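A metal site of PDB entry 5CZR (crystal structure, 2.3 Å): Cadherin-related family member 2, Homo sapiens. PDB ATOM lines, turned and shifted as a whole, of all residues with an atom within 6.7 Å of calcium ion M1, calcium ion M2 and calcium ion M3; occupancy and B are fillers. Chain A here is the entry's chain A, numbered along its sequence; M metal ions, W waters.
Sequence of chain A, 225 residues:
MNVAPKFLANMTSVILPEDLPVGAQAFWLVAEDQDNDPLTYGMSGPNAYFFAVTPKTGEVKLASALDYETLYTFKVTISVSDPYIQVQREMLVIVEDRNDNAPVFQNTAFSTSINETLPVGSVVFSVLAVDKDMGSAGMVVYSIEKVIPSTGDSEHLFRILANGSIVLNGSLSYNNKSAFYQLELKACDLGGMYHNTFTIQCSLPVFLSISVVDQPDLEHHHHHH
OD2 of Asp 97 sits at hydrogen-bond distance from N of Met 134 (2.9 Å).
O of Asn 99 lies within hydrogen-bond range of NE2 of Gln 201 (2.8 Å).
The side-chain carboxylate (OE2) of Glu 18 sits close to the backbone NH (N) of Tyr 68, 3.0 Å away.
The side-chain carboxylate of Glu 96 lies within salt-bridge range of the guanidinium group of Arg 98, at 2.9 Å.
O of Gln 201 is in hydrogen-bond range of N of Asp 189.
N of Ala 137 sits at hydrogen-bond distance from O of Gly 191 (3.3 Å).
The side-chain amide nitrogen (ND2) of Asn 101 sits close to the side-chain carboxylate (OE1) of Glu 69 (3.4 Å).
The side-chain carboxylate of Asp 100 sits close to the side-chain amide nitrogen of Asn 101 (2.8 Å).
Of the 26 residues printed, 7 come within 4 Å of calcium ion M1.
The nearest printed residue that does not touch calcium ion M1 is Asn 99 (4.7 Å).
Within 4 Å of calcium ion M2: Glu 18, Asp 67, Glu 69 and Asp 100.
The nearest printed residue that does not touch calcium ion M2 is Tyr 68 (4.1 Å).
Within 4 Å of calcium ion M3: Asn 99, Asn 101, Asp 131, Asp 133, Ala 137 and Asp 189.
The nearest printed residue that does not touch calcium ion M3 is Gln 201 (4.3 Å).
OD1 of Asp 97 binds calcium ion M1 (2.2 Å).
Calcium ion M1 is bound by OD1 of Asp 133.
Calcium ion M1 is bound by OD1 of Asp 100, 2.3 Å away.
Calcium ion M1 is bound by OE1 of Glu 18 (2.3 Å).
The side-chain carboxylate (OE2) of Glu 69 is bound to calcium ion M1 (2.4 Å).
Calcium ion M1 is bound by O of Arg 98, 2.4 Å away.
Calcium ion M1 has six donor atoms within binding distance.
Slightly farther from calcium ion M1 lies the side-chain carboxylate (OE1) of Glu 69 (2.9 Å).
Calcium ion M2 is bound by OD1 of Asp 67, water W2, water W1, OE1 of Glu 69, OD2 of Asp 100 and OE2 of Glu 18.
Calcium ion M3 is bound by O of Asn 101 (2.2 Å), OD1 of Asn 99 (2.3 Å), O of Ala 137 (2.3 Å), OD2 of Asp 189 (2.5 Å), OD2 of Asp 133 (2.5 Å), OD2 of Asp 131 (2.5 Å) and OD1 of Asp 131 (2.6 Å).
Calcium ion M3 has seven donor atoms within binding distance.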
ATOM      1  N   GLU A  18     -18.612 -20.094 -15.008  1.00  0.00           N
ATOM      2  CA  GLU A  18     -17.645 -20.506 -13.989  1.00  0.00           C
ATOM      3  C   GLU A  18     -18.202 -21.607 -13.061  1.00  0.00           C
ATOM      4  O   GLU A  18     -17.429 -22.343 -12.485  1.00  0.00           O
ATOM      5  CB  GLU A  18     -17.117 -19.320 -13.162  1.00  0.00           C
ATOM      6  CG  GLU A  18     -18.161 -18.607 -12.305  1.00  0.00           C
ATOM      7  CD  GLU A  18     -17.555 -17.745 -11.217  1.00  0.00           C
ATOM      8  OE1 GLU A  18     -18.123 -16.680 -10.938  1.00  0.00           O
ATOM      9  OE2 GLU A  18     -16.517 -18.148 -10.642  1.00  0.00           O
ATOM     10  N   LEU A  66     -13.702 -24.540 -12.950  1.00  0.00           N
ATOM     11  CA  LEU A  66     -13.453 -23.175 -13.374  1.00  0.00           C
ATOM     12  C   LEU A  66     -13.643 -22.219 -12.213  1.00  0.00           C
ATOM     13  O   LEU A  66     -14.302 -22.563 -11.237  1.00  0.00           O
ATOM     14  CB  LEU A  66     -14.408 -22.777 -14.515  1.00  0.00           C
ATOM     15  CG  LEU A  66     -14.401 -23.708 -15.749  1.00  0.00           C
ATOM     16  CD1 LEU A  66     -15.455 -23.278 -16.764  1.00  0.00           C
ATOM     17  CD2 LEU A  66     -13.020 -23.699 -16.415  1.00  0.00           C
ATOM     18  N   ASP A  67     -13.116 -21.010 -12.338  1.00  0.00           N
ATOM     19  CA  ASP A  67     -13.390 -19.929 -11.354  1.00  0.00           C
ATOM     20  C   ASP A  67     -13.032 -18.584 -11.964  1.00  0.00           C
ATOM     21  O   ASP A  67     -11.867 -18.331 -12.261  1.00  0.00           O
ATOM     22  CB  ASP A  67     -12.608 -20.169 -10.054  1.00  0.00           C
ATOM     23  CG  ASP A  67     -12.843 -19.113  -9.003  1.00  0.00           C
ATOM     24  OD1 ASP A  67     -13.721 -18.241  -9.192  1.00  0.00           O
ATOM     25  OD2 ASP A  67     -12.154 -19.149  -7.953  1.00  0.00           O
ATOM     26  N   TYR A  68     -14.048 -17.769 -12.224  1.00  0.00           N
ATOM     27  CA  TYR A  68     -13.867 -16.438 -12.820  1.00  0.00           C
ATOM     28  C   TYR A  68     -12.937 -15.588 -11.964  1.00  0.00           C
ATOM     29  O   TYR A  68     -12.162 -14.801 -12.494  1.00  0.00           O
ATOM     30  CB  TYR A  68     -15.217 -15.724 -12.967  1.00  0.00           C
ATOM     31  CG  TYR A  68     -15.118 -14.381 -13.630  1.00  0.00           C
ATOM     32  CD1 TYR A  68     -15.221 -14.249 -15.031  1.00  0.00           C
ATOM     33  CD2 TYR A  68     -14.939 -13.236 -12.876  1.00  0.00           C
ATOM     34  CE1 TYR A  68     -15.122 -13.010 -15.662  1.00  0.00           C
ATOM     35  CE2 TYR A  68     -14.835 -11.980 -13.485  1.00  0.00           C
ATOM     36  CZ  TYR A  68     -14.932 -11.872 -14.869  1.00  0.00           C
ATOM     37  OH  TYR A  68     -14.822 -10.640 -15.440  1.00  0.00           O
ATOM     38  N   GLU A  69     -12.992 -15.771 -10.642  1.00  0.00           N
ATOM     39  CA  GLU A  69     -12.247 -14.937  -9.731  1.00  0.00           C
ATOM     40  C   GLU A  69     -10.743 -15.270  -9.757  1.00  0.00           C
ATOM     41  O   GLU A  69      -9.955 -14.529  -9.217  1.00  0.00           O
ATOM     42  CB  GLU A  69     -12.809 -15.070  -8.299  1.00  0.00           C
ATOM     43  CG  GLU A  69     -14.072 -14.244  -8.018  1.00  0.00           C
ATOM     44  CD  GLU A  69     -15.324 -14.718  -8.732  1.00  0.00           C
ATOM     45  OE1 GLU A  69     -15.618 -15.905  -8.743  1.00  0.00           O
ATOM     46  OE2 GLU A  69     -16.078 -13.895  -9.291  1.00  0.00           O
ATOM     47  N   THR A  70     -10.376 -16.378 -10.395  1.00  0.00           N
ATOM     48  CA  THR A  70      -8.992 -16.906 -10.353  1.00  0.00           C
ATOM     49  C   THR A  70      -8.333 -16.900 -11.739  1.00  0.00           C
ATOM     50  O   THR A  70      -7.165 -16.580 -11.849  1.00  0.00           O
ATOM     51  CB  THR A  70      -9.033 -18.299  -9.747  1.00  0.00           C
ATOM     52  OG1 THR A  70      -9.155 -18.147  -8.335  1.00  0.00           O
ATOM     53  CG2 THR A  70      -7.793 -19.141 -10.029  1.00  0.00           C
ATOM     54  N   GLU A  96     -17.394 -17.066 -17.882  1.00  0.00           N
ATOM     55  CA  GLU A  96     -18.390 -16.074 -17.435  1.00  0.00           C
ATOM     56  C   GLU A  96     -18.553 -16.044 -15.921  1.00  0.00           C
ATOM     57  O   GLU A  96     -18.588 -17.084 -15.255  1.00  0.00           O
ATOM     58  CB  GLU A  96     -19.734 -16.330 -18.057  1.00  0.00           C
ATOM     59  CG  GLU A  96     -19.784 -15.887 -19.524  1.00  0.00           C
ATOM     60  CD  GLU A  96     -21.194 -15.729 -20.138  1.00  0.00           C
ATOM     61  OE1 GLU A  96     -22.156 -16.367 -19.680  1.00  0.00           O
ATOM     62  OE2 GLU A  96     -21.323 -14.997 -21.136  1.00  0.00           O
ATOM     63  N   ASP A  97     -18.617 -14.831 -15.384  1.00  0.00           N
ATOM     64  CA  ASP A  97     -18.839 -14.616 -13.973  1.00  0.00           C
ATOM     65  C   ASP A  97     -20.245 -15.057 -13.615  1.00  0.00           C
ATOM     66  O   ASP A  97     -21.194 -14.826 -14.338  1.00  0.00           O
ATOM     67  CB  ASP A  97     -18.622 -13.150 -13.625  1.00  0.00           C
ATOM     68  CG  ASP A  97     -18.735 -12.872 -12.142  1.00  0.00           C
ATOM     69  OD1 ASP A  97     -18.217 -13.665 -11.302  1.00  0.00           O
ATOM     70  OD2 ASP A  97     -19.368 -11.838 -11.803  1.00  0.00           O
ATOM     71  N   ARG A  98     -20.360 -15.677 -12.459  1.00  0.00           N
ATOM     72  CA  ARG A  98     -21.647 -15.986 -11.892  1.00  0.00           C
ATOM     73  C   ARG A  98     -21.664 -15.438 -10.459  1.00  0.00           C
ATOM     74  O   ARG A  98     -20.612 -15.051  -9.908  1.00  0.00           O
ATOM     75  CB  ARG A  98     -21.869 -17.506 -11.924  1.00  0.00           C
ATOM     76  CG  ARG A  98     -22.027 -18.110 -13.336  1.00  0.00           C
ATOM     77  CD  ARG A  98     -23.396 -17.730 -13.882  1.00  0.00           C
ATOM     78  NE  ARG A  98     -23.648 -18.008 -15.284  1.00  0.00           N
ATOM     79  CZ  ARG A  98     -23.453 -17.152 -16.272  1.00  0.00           C
ATOM     80  NH1 ARG A  98     -22.960 -15.941 -16.064  1.00  0.00           N
ATOM     81  NH2 ARG A  98     -23.727 -17.532 -17.480  1.00  0.00           N
ATOM     82  N   ASN A  99     -22.856 -15.412  -9.847  1.00  0.00           N
ATOM     83  CA  ASN A  99     -22.979 -14.813  -8.507  1.00  0.00           C
ATOM     84  C   ASN A  99     -22.646 -15.773  -7.374  1.00  0.00           C
ATOM     85  O   ASN A  99     -23.542 -16.212  -6.630  1.00  0.00           O
ATOM     86  CB  ASN A  99     -24.354 -14.202  -8.311  1.00  0.00           C
ATOM     87  CG  ASN A  99     -24.419 -13.350  -7.082  1.00  0.00           C
ATOM     88  OD1 ASN A  99     -23.390 -12.968  -6.550  1.00  0.00           O
ATOM     89  ND2 ASN A  99     -25.635 -13.008  -6.643  1.00  0.00           N
ATOM     90  N   ASP A 100     -21.376 -16.090  -7.231  1.00  0.00           N
ATOM     91  CA  ASP A 100     -20.910 -17.106  -6.287  1.00  0.00           C
ATOM     92  C   ASP A 100     -20.157 -16.543  -5.068  1.00  0.00           C
ATOM     93  O   ASP A 100     -19.635 -17.315  -4.257  1.00  0.00           O
ATOM     94  CB  ASP A 100     -20.016 -18.126  -7.005  1.00  0.00           C
ATOM     95  CG  ASP A 100     -18.768 -17.509  -7.594  1.00  0.00           C
ATOM     96  OD1 ASP A 100     -18.647 -16.245  -7.692  1.00  0.00           O
ATOM     97  OD2 ASP A 100     -17.879 -18.299  -7.961  1.00  0.00           O
ATOM     98  N   ASN A 101     -20.124 -15.217  -4.937  1.00  0.00           N
ATOM     99  CA  ASN A 101     -19.610 -14.568  -3.753  1.00  0.00           C
ATOM    100  C   ASN A 101     -20.648 -13.688  -3.084  1.00  0.00           C
ATOM    101  O   ASN A 101     -21.565 -13.132  -3.720  1.00  0.00           O
ATOM    102  CB  ASN A 101     -18.407 -13.732  -4.132  1.00  0.00           C
ATOM    103  CG  ASN A 101     -17.222 -14.561  -4.552  1.00  0.00           C
ATOM    104  OD1 ASN A 101     -16.455 -14.998  -3.719  1.00  0.00           O
ATOM    105  ND2 ASN A 101     -17.111 -14.844  -5.844  1.00  0.00           N
ATOM    106  N   ALA A 102     -20.487 -13.568  -1.783  1.00  0.00           N
ATOM    107  CA  ALA A 102     -21.370 -12.764  -0.954  1.00  0.00           C
ATOM    108  C   ALA A 102     -20.598 -11.496  -0.540  1.00  0.00           C
ATOM    109  O   ALA A 102     -19.378 -11.498  -0.478  1.00  0.00           O
ATOM    110  CB  ALA A 102     -21.763 -13.556   0.287  1.00  0.00           C
ATOM    111  N   PRO A 103     -21.314 -10.412  -0.214  1.00  0.00           N
ATOM    112  CA  PRO A 103     -20.599  -9.312   0.409  1.00  0.00           C
ATOM    113  C   PRO A 103     -19.926  -9.686   1.752  1.00  0.00           C
ATOM    114  O   PRO A 103     -20.486 -10.437   2.539  1.00  0.00           O
ATOM    115  CB  PRO A 103     -21.690  -8.282   0.621  1.00  0.00           C
ATOM    116  CG  PRO A 103     -22.755  -8.631  -0.369  1.00  0.00           C
ATOM    117  CD  PRO A 103     -22.737 -10.131  -0.396  1.00  0.00           C
ATOM    118  N   ASP A 131     -18.033  -7.137  -2.370  1.00  0.00           N
ATOM    119  CA  ASP A 131     -18.411  -8.366  -3.064  1.00  0.00           C
ATOM    120  C   ASP A 131     -17.564  -8.472  -4.315  1.00  0.00           C
ATOM    121  O   ASP A 131     -17.568  -7.575  -5.153  1.00  0.00           O
ATOM    122  CB  ASP A 131     -19.881  -8.265  -3.431  1.00  0.00           C
ATOM    123  CG  ASP A 131     -20.459  -9.556  -3.964  1.00  0.00           C
ATOM    124  OD1 ASP A 131     -19.965 -10.075  -4.988  1.00  0.00           O
ATOM    125  OD2 ASP A 131     -21.486  -9.992  -3.416  1.00  0.00           O
ATOM    126  N   LYS A 132     -16.867  -9.586  -4.472  1.00  0.00           N
ATOM    127  CA  LYS A 132     -15.955  -9.797  -5.603  1.00  0.00           C
ATOM    128  C   LYS A 132     -16.577  -9.893  -6.997  1.00  0.00           C
ATOM    129  O   LYS A 132     -15.887  -9.687  -7.996  1.00  0.00           O
ATOM    130  CB  LYS A 132     -15.187 -11.098  -5.397  1.00  0.00           C
ATOM    131  CG  LYS A 132     -14.218 -11.050  -4.228  1.00  0.00           C
ATOM    132  CD  LYS A 132     -13.822 -12.460  -3.828  1.00  0.00           C
ATOM    133  CE  LYS A 132     -12.878 -12.440  -2.632  1.00  0.00           C
ATOM    134  NZ  LYS A 132     -12.213 -13.760  -2.544  1.00  0.00           N
ATOM    135  N   ASP A 133     -17.849 -10.227  -7.076  1.00  0.00           N
ATOM    136  CA  ASP A 133     -18.470 -10.485  -8.363  1.00  0.00           C
ATOM    137  C   ASP A 133     -18.596  -9.204  -9.174  1.00  0.00           C
ATOM    138  O   ASP A 133     -18.412  -8.125  -8.647  1.00  0.00           O
ATOM    139  CB  ASP A 133     -19.824 -11.170  -8.178  1.00  0.00           C
ATOM    140  CG  ASP A 133     -19.684 -12.545  -7.515  1.00  0.00           C
ATOM    141  OD1 ASP A 133     -18.807 -13.329  -7.931  1.00  0.00           O
ATOM    142  OD2 ASP A 133     -20.426 -12.839  -6.563  1.00  0.00           O
ATOM    143  N   MET A 134     -18.827  -9.359 -10.485  1.00  0.00           N
ATOM    144  CA  MET A 134     -18.997  -8.253 -11.430  1.00  0.00           C
ATOM    145  C   MET A 134     -20.461  -7.796 -11.526  1.00  0.00           C
ATOM    146  O   MET A 134     -21.380  -8.533 -11.228  1.00  0.00           O
ATOM    147  CB  MET A 134     -18.515  -8.690 -12.828  1.00  0.00           C
ATOM    148  CG  MET A 134     -17.023  -9.068 -12.908  1.00  0.00           C
ATOM    149  SD  MET A 134     -15.957  -7.672 -12.461  1.00  0.00           S
ATOM    150  CE  MET A 134     -14.352  -8.386 -12.754  1.00  0.00           C
ATOM    151  N   SER A 136     -24.127  -6.325 -11.265  1.00  0.00           N
ATOM    152  CA  SER A 136     -25.105  -6.269 -10.185  1.00  0.00           C
ATOM    153  C   SER A 136     -24.777  -7.285  -9.117  1.00  0.00           C
ATOM    154  O   SER A 136     -25.095  -7.083  -7.935  1.00  0.00           O
ATOM    155  CB  SER A 136     -26.497  -6.585 -10.690  1.00  0.00           C
ATOM    156  OG  SER A 136     -26.850  -5.614 -11.640  1.00  0.00           O
ATOM    157  N   ALA A 137     -24.153  -8.393  -9.542  1.00  0.00           N
ATOM    158  CA  ALA A 137     -23.786  -9.439  -8.598  1.00  0.00           C
ATOM    159  C   ALA A 137     -22.731  -8.997  -7.580  1.00  0.00           C
ATOM    160  O   ALA A 137     -22.531  -9.695  -6.561  1.00  0.00           O
ATOM    161  CB  ALA A 137     -23.338 -10.667  -9.359  1.00  0.00           C
ATOM    162  N   GLY A 138     -22.057  -7.879  -7.868  1.00  0.00           N
ATOM    163  CA  GLY A 138     -21.104  -7.262  -6.982  1.00  0.00           C
ATOM    164  C   GLY A 138     -21.525  -5.927  -6.343  1.00  0.00           C
ATOM    165  O   GLY A 138     -20.743  -5.366  -5.577  1.00  0.00           O
ATOM    166  N   MET A 139     -22.725  -5.427  -6.674  1.00  0.00           N
ATOM    167  CA  MET A 139     -23.237  -4.172  -6.080  1.00  0.00           C
ATOM    168  C   MET A 139     -23.850  -4.483  -4.731  1.00  0.00           C
ATOM    169  O   MET A 139     -24.702  -5.346  -4.587  1.00  0.00           O
ATOM    170  CB  MET A 139     -24.249  -3.471  -6.992  1.00  0.00           C
ATOM    171  CG  MET A 139     -23.643  -2.827  -8.252  1.00  0.00           C
ATOM    172  SD  MET A 139     -24.806  -2.013  -9.401  1.00  0.00           S
ATOM    173  CE  MET A 139     -23.896  -1.842 -10.962  1.00  0.00           C
ATOM    174  N   ASP A 189     -25.964  -8.494  -2.304  1.00  0.00           N
ATOM    175  CA  ASP A 189     -25.744  -8.003  -3.675  1.00  0.00           C
ATOM    176  C   ASP A 189     -27.090  -7.786  -4.306  1.00  0.00           C
ATOM    177  O   ASP A 189     -28.096  -8.087  -3.698  1.00  0.00           O
ATOM    178  CB  ASP A 189     -24.809  -8.900  -4.513  1.00  0.00           C
ATOM    179  CG  ASP A 189     -25.254 -10.347  -4.592  1.00  0.00           C
ATOM    180  OD1 ASP A 189     -26.478 -10.622  -4.767  1.00  0.00           O
ATOM    181  OD2 ASP A 189     -24.396 -11.248  -4.495  1.00  0.00           O
ATOM    182  N   LEU A 190     -27.131  -7.261  -5.526  1.00  0.00           N
ATOM    183  CA  LEU A 190     -28.385  -7.105  -6.286  1.00  0.00           C
ATOM    184  C   LEU A 190     -28.710  -8.291  -7.140  1.00  0.00           C
ATOM    185  O   LEU A 190     -29.648  -8.284  -7.922  1.00  0.00           O
ATOM    186  CB  LEU A 190     -28.325  -5.849  -7.165  1.00  0.00           C
ATOM    187  CG  LEU A 190     -28.345  -4.543  -6.351  1.00  0.00           C
ATOM    188  CD1 LEU A 190     -28.087  -3.358  -7.263  1.00  0.00           C
ATOM    189  CD2 LEU A 190     -29.668  -4.398  -5.594  1.00  0.00           C
ATOM    190  N   GLY A 191     -27.916  -9.357  -6.994  1.00  0.00           N
ATOM    191  CA  GLY A 191     -28.249 -10.632  -7.624  1.00  0.00           C
ATOM    192  C   GLY A 191     -27.648 -10.849  -9.007  1.00  0.00           C
ATOM    193  O   GLY A 191     -27.073  -9.930  -9.620  1.00  0.00           O
ATOM    194  N   GLN A 201     -27.001 -12.979  -2.963  1.00  0.00           N
ATOM    195  CA  GLN A 201     -26.101 -13.383  -1.861  1.00  0.00           C
ATOM    196  C   GLN A 201     -26.051 -12.338  -0.790  1.00  0.00           C
ATOM    197  O   GLN A 201     -25.999 -11.155  -1.102  1.00  0.00           O
ATOM    198  CB  GLN A 201     -24.665 -13.634  -2.359  1.00  0.00           C
ATOM    199  CG  GLN A 201     -24.560 -14.603  -3.519  1.00  0.00           C
ATOM    200  CD  GLN A 201     -24.498 -16.058  -3.062  1.00  0.00           C
ATOM    201  OE1 GLN A 201     -24.743 -16.372  -1.906  1.00  0.00           O
ATOM    202  NE2 GLN A 201     -24.160 -16.953  -3.972  1.00  0.00           N
HETATM  203 CA    CA M   1     -18.238 -14.858  -9.505  1.00  0.00          CA
HETATM  204 CA    CA M   2     -15.700 -18.121  -8.527  1.00  0.00          CA
HETATM  205 CA    CA M   3     -22.076 -11.569  -5.238  1.00  0.00          CA
HETATM  206  O   HOH W   1     -15.680 -20.335  -8.344  1.00  0.00           O
HETATM  207  O   HOH W   2     -15.542 -17.580  -6.427  1.00  0.00           O
